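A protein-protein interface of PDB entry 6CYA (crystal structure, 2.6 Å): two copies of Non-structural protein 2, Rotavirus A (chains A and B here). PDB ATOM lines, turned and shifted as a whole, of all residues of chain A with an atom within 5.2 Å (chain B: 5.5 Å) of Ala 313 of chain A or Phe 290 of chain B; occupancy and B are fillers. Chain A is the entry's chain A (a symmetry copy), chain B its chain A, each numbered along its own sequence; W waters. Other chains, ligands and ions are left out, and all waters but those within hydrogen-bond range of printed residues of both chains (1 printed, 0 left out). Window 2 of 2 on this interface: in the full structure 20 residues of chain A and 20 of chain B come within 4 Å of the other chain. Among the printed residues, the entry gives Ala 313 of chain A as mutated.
Of the 10 printed residues of chain B, 4 touch a printed residue of chain A.
Printed residues of chain B that touch a printed residue of chain A: Ser 232, Asn 268, Leu 289 and Phe 290.
Hydrophobic or aromatic side chains of chain A that line the printed part of chain B: Met 309 and Val 312.
Among the printed residues, merely in contact across the chains: Met 309 of chain A with Asn 268 of chain B (3.8 Å), Met 309 of chain A with Leu 289 of chain B (3.2 Å), Met 309 of chain A with Phe 290 of chain B (3.2 Å), Glu 311 of chain A with Ser 232 of chain B (3.2 Å), Val 312 of chain A with Leu 289 of chain B (3.8 Å), Val 312 of chain A with Phe 290 of chain B (3.4 Å) and Ala 313 of chain A with Phe 290 of chain B (3.8 Å).
Of the printed residues of chain A, Phe 290 of chain B touches Met 309 (3.2 Å), Val 312 (3.4 Å) and Ala 313 (3.8 Å).
Of the printed residues of chain B, Val 312 of chain A touches Leu 289 (3.8 Å) and Phe 290 (3.4 Å).
Printed residues of chain B within 4 Å of Met 309 of chain A: Asn 268 (3.8 Å), Leu 289 (3.2 Å) and Phe 290 (3.2 Å).
Arg 287 of chain B touches none of the printed residues of chain A.
Gln 291 of chain B touches none of the printed residues of chain A.
The nearest printed residue of chain A that does not touch Phe 290 of chain B is Gln 314 of chain A (5.5 Å).
No position is printed for both chains.
Of the 7 pairs that touch across the chains among the printed residues, none has its exchanged pair printed and touching as well.
Water W1 lies within hydrogen-bond range of O of Val 312 of chain A (2.7 Å), O of Ser 232 of chain B (2.9 Å) and N of Ala 235 of chain B (3.0 Å).
The backbone carbonyl oxygen of Leu 288 of chain B lies within hydrogen-bond range of the side-chain amide nitrogen of Asn 268 of chain B.
The backbone carbonyl oxygen (O) of Leu 289 of chain B sits at hydrogen-bond distance from the side-chain amide nitrogen (ND2) of Asn 268 of chain B (2.9 Å).
The side-chain amide nitrogen (ND2) of Asn 268 of chain B is in hydrogen-bond range of the backbone carbonyl oxygen (O) of Gln 291 of chain B.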
ATOM      1  N   MET A 309      17.184  -0.481 -11.210  1.00  0.00           N
ATOM      2  CA  MET A 309      17.624  -1.173 -10.002  1.00  0.00           C
ATOM      3  C   MET A 309      18.487  -2.386 -10.324  1.00  0.00           C
ATOM      4  O   MET A 309      19.383  -2.728  -9.543  1.00  0.00           O
ATOM      5  CB  MET A 309      16.421  -1.586  -9.156  1.00  0.00           C
ATOM      6  CG  MET A 309      15.572  -0.420  -8.695  1.00  0.00           C
ATOM      7  SD  MET A 309      16.541   0.847  -7.853  1.00  0.00           S
ATOM      8  CE  MET A 309      17.298  -0.110  -6.547  1.00  0.00           C
ATOM      9  N   ASP A 310      18.240  -3.047 -11.458  1.00  0.00           N
ATOM     10  CA  ASP A 310      19.124  -4.130 -11.873  1.00  0.00           C
ATOM     11  C   ASP A 310      20.513  -3.612 -12.226  1.00  0.00           C
ATOM     12  O   ASP A 310      21.490  -4.364 -12.148  1.00  0.00           O
ATOM     13  CB  ASP A 310      18.519  -4.884 -13.056  1.00  0.00           C
ATOM     14  CG  ASP A 310      17.254  -5.634 -12.686  1.00  0.00           C
ATOM     15  OD1 ASP A 310      17.018  -5.851 -11.479  1.00  0.00           O
ATOM     16  OD2 ASP A 310      16.499  -6.016 -13.604  1.00  0.00           O
ATOM     17  N   GLU A 311      20.622  -2.339 -12.616  1.00  0.00           N
ATOM     18  CA  GLU A 311      21.930  -1.744 -12.872  1.00  0.00           C
ATOM     19  C   GLU A 311      22.627  -1.357 -11.574  1.00  0.00           C
ATOM     20  O   GLU A 311      23.847  -1.509 -11.454  1.00  0.00           O
ATOM     21  CB  GLU A 311      21.788  -0.524 -13.781  1.00  0.00           C
ATOM     22  CG  GLU A 311      21.151  -0.819 -15.124  1.00  0.00           C
ATOM     23  CD  GLU A 311      22.173  -1.134 -16.195  1.00  0.00           C
ATOM     24  OE1 GLU A 311      21.777  -1.643 -17.265  1.00  0.00           O
ATOM     25  OE2 GLU A 311      23.373  -0.875 -15.964  1.00  0.00           O
ATOM     26  N   VAL A 312      21.872  -0.846 -10.597  1.00  0.00           N
ATOM     27  CA  VAL A 312      22.455  -0.520  -9.298  1.00  0.00           C
ATOM     28  C   VAL A 312      23.043  -1.768  -8.652  1.00  0.00           C
ATOM     29  O   VAL A 312      24.133  -1.730  -8.069  1.00  0.00           O
ATOM     30  CB  VAL A 312      21.407   0.156  -8.396  1.00  0.00           C
ATOM     31  CG1 VAL A 312      21.987   0.438  -7.018  1.00  0.00           C
ATOM     32  CG2 VAL A 312      20.911   1.438  -9.046  1.00  0.00           C
ATOM     33  N   ALA A 313      22.338  -2.892  -8.748  1.00  0.00           N
ATOM     34  CA  ALA A 313      22.931  -4.179  -8.426  1.00  0.00           C
ATOM     35  C   ALA A 313      23.792  -4.656  -9.595  1.00  0.00           C
ATOM     36  O   ALA A 313      23.745  -4.108 -10.698  1.00  0.00           O
ATOM     37  CB  ALA A 313      21.848  -5.204  -8.095  1.00  0.00           C
ATOM     38  N   GLN A 314      24.589  -5.692  -9.346  1.00  0.00           N
ATOM     39  CA  GLN A 314      25.530  -6.215 -10.344  1.00  0.00           C
ATOM     40  C   GLN A 314      26.472  -5.132 -10.872  1.00  0.00           C
ATOM     41  O   GLN A 314      26.633  -4.072 -10.264  1.00  0.00           O
ATOM     42  CB  GLN A 314      24.788  -6.860 -11.521  1.00  0.00           C
ATOM     43  CG  GLN A 314      23.530  -7.622 -11.142  1.00  0.00           C
ATOM     44  CD  GLN A 314      22.535  -7.683 -12.284  1.00  0.00           C
ATOM     45  OE1 GLN A 314      22.851  -7.316 -13.416  1.00  0.00           O
ATOM     46  NE2 GLN A 314      21.325  -8.145 -11.991  1.00  0.00           N
ATOM     47  N   SER B 232      25.336   1.645 -12.717  1.00  0.00           N
ATOM     48  CA  SER B 232      26.117   0.435 -12.485  1.00  0.00           C
ATOM     49  C   SER B 232      27.313   0.679 -11.575  1.00  0.00           C
ATOM     50  O   SER B 232      27.894  -0.284 -11.064  1.00  0.00           O
ATOM     51  CB  SER B 232      26.591  -0.150 -13.815  1.00  0.00           C
ATOM     52  OG  SER B 232      27.345   0.800 -14.550  1.00  0.00           O
ATOM     53  N   ALA B 235      27.081   1.873  -6.610  1.00  0.00           N
ATOM     54  CA  ALA B 235      27.410   1.080  -5.430  1.00  0.00           C
ATOM     55  C   ALA B 235      28.856   1.307  -5.004  1.00  0.00           C
ATOM     56  O   ALA B 235      29.153   1.371  -3.805  1.00  0.00           O
ATOM     57  CB  ALA B 235      27.150  -0.401  -5.700  1.00  0.00           C
ATOM     58  N   ASN B 268      17.296   7.123  -3.700  1.00  0.00           N
ATOM     59  CA  ASN B 268      17.997   6.100  -2.929  1.00  0.00           C
ATOM     60  C   ASN B 268      19.302   6.635  -2.351  1.00  0.00           C
ATOM     61  O   ASN B 268      19.669   6.303  -1.218  1.00  0.00           O
ATOM     62  CB  ASN B 268      18.263   4.873  -3.799  1.00  0.00           C
ATOM     63  CG  ASN B 268      16.985   4.195  -4.255  1.00  0.00           C
ATOM     64  OD1 ASN B 268      16.026   4.855  -4.654  1.00  0.00           O
ATOM     65  ND2 ASN B 268      16.966   2.868  -4.195  1.00  0.00           N
ATOM     66  N   LYS B 286      23.517   0.995   3.073  1.00  0.00           N
ATOM     67  CA  LYS B 286      23.768   0.591   1.694  1.00  0.00           C
ATOM     68  C   LYS B 286      22.637  -0.266   1.137  1.00  0.00           C
ATOM     69  O   LYS B 286      22.412  -0.270  -0.078  1.00  0.00           O
ATOM     70  CB  LYS B 286      25.096  -0.159   1.581  1.00  0.00           C
ATOM     71  CG  LYS B 286      25.689  -0.130   0.185  1.00  0.00           C
ATOM     72  CD  LYS B 286      27.072  -0.752   0.142  1.00  0.00           C
ATOM     73  CE  LYS B 286      27.472  -1.069  -1.291  1.00  0.00           C
ATOM     74  NZ  LYS B 286      28.810  -1.715  -1.371  1.00  0.00           N
ATOM     75  N   ARG B 287      21.916  -0.989   1.998  1.00  0.00           N
ATOM     76  CA  ARG B 287      20.760  -1.745   1.529  1.00  0.00           C
ATOM     77  C   ARG B 287      19.663  -0.828   1.003  1.00  0.00           C
ATOM     78  O   ARG B 287      18.810  -1.278   0.228  1.00  0.00           O
ATOM     79  CB  ARG B 287      20.217  -2.637   2.651  1.00  0.00           C
ATOM     80  CG  ARG B 287      21.001  -3.933   2.843  1.00  0.00           C
ATOM     81  CD  ARG B 287      20.290  -4.897   3.783  1.00  0.00           C
ATOM     82  NE  ARG B 287      20.248  -4.412   5.161  1.00  0.00           N
ATOM     83  CZ  ARG B 287      20.985  -4.905   6.154  1.00  0.00           C
ATOM     84  NH1 ARG B 287      21.831  -5.901   5.930  1.00  0.00           N
ATOM     85  NH2 ARG B 287      20.875  -4.399   7.374  1.00  0.00           N
ATOM     86  N   LEU B 288      19.678   0.449   1.395  1.00  0.00           N
ATOM     87  CA  LEU B 288      18.716   1.412   0.873  1.00  0.00           C
ATOM     88  C   LEU B 288      19.008   1.799  -0.571  1.00  0.00           C
ATOM     89  O   LEU B 288      18.111   2.297  -1.258  1.00  0.00           O
ATOM     90  CB  LEU B 288      18.695   2.654   1.762  1.00  0.00           C
ATOM     91  CG  LEU B 288      18.284   2.364   3.206  1.00  0.00           C
ATOM     92  CD1 LEU B 288      18.456   3.589   4.098  1.00  0.00           C
ATOM     93  CD2 LEU B 288      16.850   1.858   3.245  1.00  0.00           C
ATOM     94  N   LEU B 289      20.241   1.585  -1.044  1.00  0.00           N
ATOM     95  CA  LEU B 289      20.536   1.792  -2.459  1.00  0.00           C
ATOM     96  C   LEU B 289      19.797   0.786  -3.329  1.00  0.00           C
ATOM     97  O   LEU B 289      19.309   1.134  -4.411  1.00  0.00           O
ATOM     98  CB  LEU B 289      22.037   1.678  -2.717  1.00  0.00           C
ATOM     99  CG  LEU B 289      23.009   2.803  -2.374  1.00  0.00           C
ATOM    100  CD1 LEU B 289      24.325   2.508  -3.059  1.00  0.00           C
ATOM    101  CD2 LEU B 289      22.472   4.161  -2.794  1.00  0.00           C
ATOM    102  N   PHE B 290      19.719  -0.467  -2.879  1.00  0.00           N
ATOM    103  CA  PHE B 290      19.210  -1.557  -3.702  1.00  0.00           C
ATOM    104  C   PHE B 290      17.718  -1.794  -3.543  1.00  0.00           C
ATOM    105  O   PHE B 290      17.122  -2.472  -4.388  1.00  0.00           O
ATOM    106  CB  PHE B 290      19.955  -2.852  -3.376  1.00  0.00           C
ATOM    107  CG  PHE B 290      21.444  -2.744  -3.517  1.00  0.00           C
ATOM    108  CD1 PHE B 290      22.043  -2.846  -4.761  1.00  0.00           C
ATOM    109  CD2 PHE B 290      22.243  -2.533  -2.407  1.00  0.00           C
ATOM    110  CE1 PHE B 290      23.411  -2.746  -4.896  1.00  0.00           C
ATOM    111  CE2 PHE B 290      23.614  -2.430  -2.534  1.00  0.00           C
ATOM    112  CZ  PHE B 290      24.198  -2.537  -3.780  1.00  0.00           C
ATOM    113  N   GLN B 291      17.101  -1.272  -2.489  1.00  0.00           N
ATOM    114  CA  GLN B 291      15.670  -1.441  -2.293  1.00  0.00           C
ATOM    115  C   GLN B 291      14.937  -0.352  -3.062  1.00  0.00           C
ATOM    116  O   GLN B 291      15.335   0.818  -3.036  1.00  0.00           O
ATOM    117  CB  GLN B 291      15.314  -1.423  -0.801  1.00  0.00           C
ATOM    118  CG  GLN B 291      14.823  -0.100  -0.237  1.00  0.00           C
ATOM    119  CD  GLN B 291      14.502  -0.187   1.243  1.00  0.00           C
ATOM    120  OE1 GLN B 291      15.068  -1.009   1.966  1.00  0.00           O
ATOM    121  NE2 GLN B 291      13.590   0.663   1.703  1.00  0.00           N
ATOM    122  N   LYS B 292      13.899  -0.749  -3.789  1.00  0.00           N
ATOM    123  CA  LYS B 292      13.141   0.188  -4.610  1.00  0.00           C
ATOM    124  C   LYS B 292      12.135   0.897  -3.717  1.00  0.00           C
ATOM    125  O   LYS B 292      11.121   0.323  -3.317  1.00  0.00           O
ATOM    126  CB  LYS B 292      12.453  -0.531  -5.765  1.00  0.00           C
ATOM    127  CG  LYS B 292      11.287   0.238  -6.382  1.00  0.00           C
ATOM    128  CD  LYS B 292      10.635  -0.541  -7.514  1.00  0.00           C
ATOM    129  CE  LYS B 292      10.595  -2.031  -7.223  1.00  0.00           C
ATOM    130  NZ  LYS B 292      10.297  -2.825  -8.447  1.00  0.00           N
HETATM  131  O   HOH W   1      26.087   0.031  -8.807  1.00  0.00           O
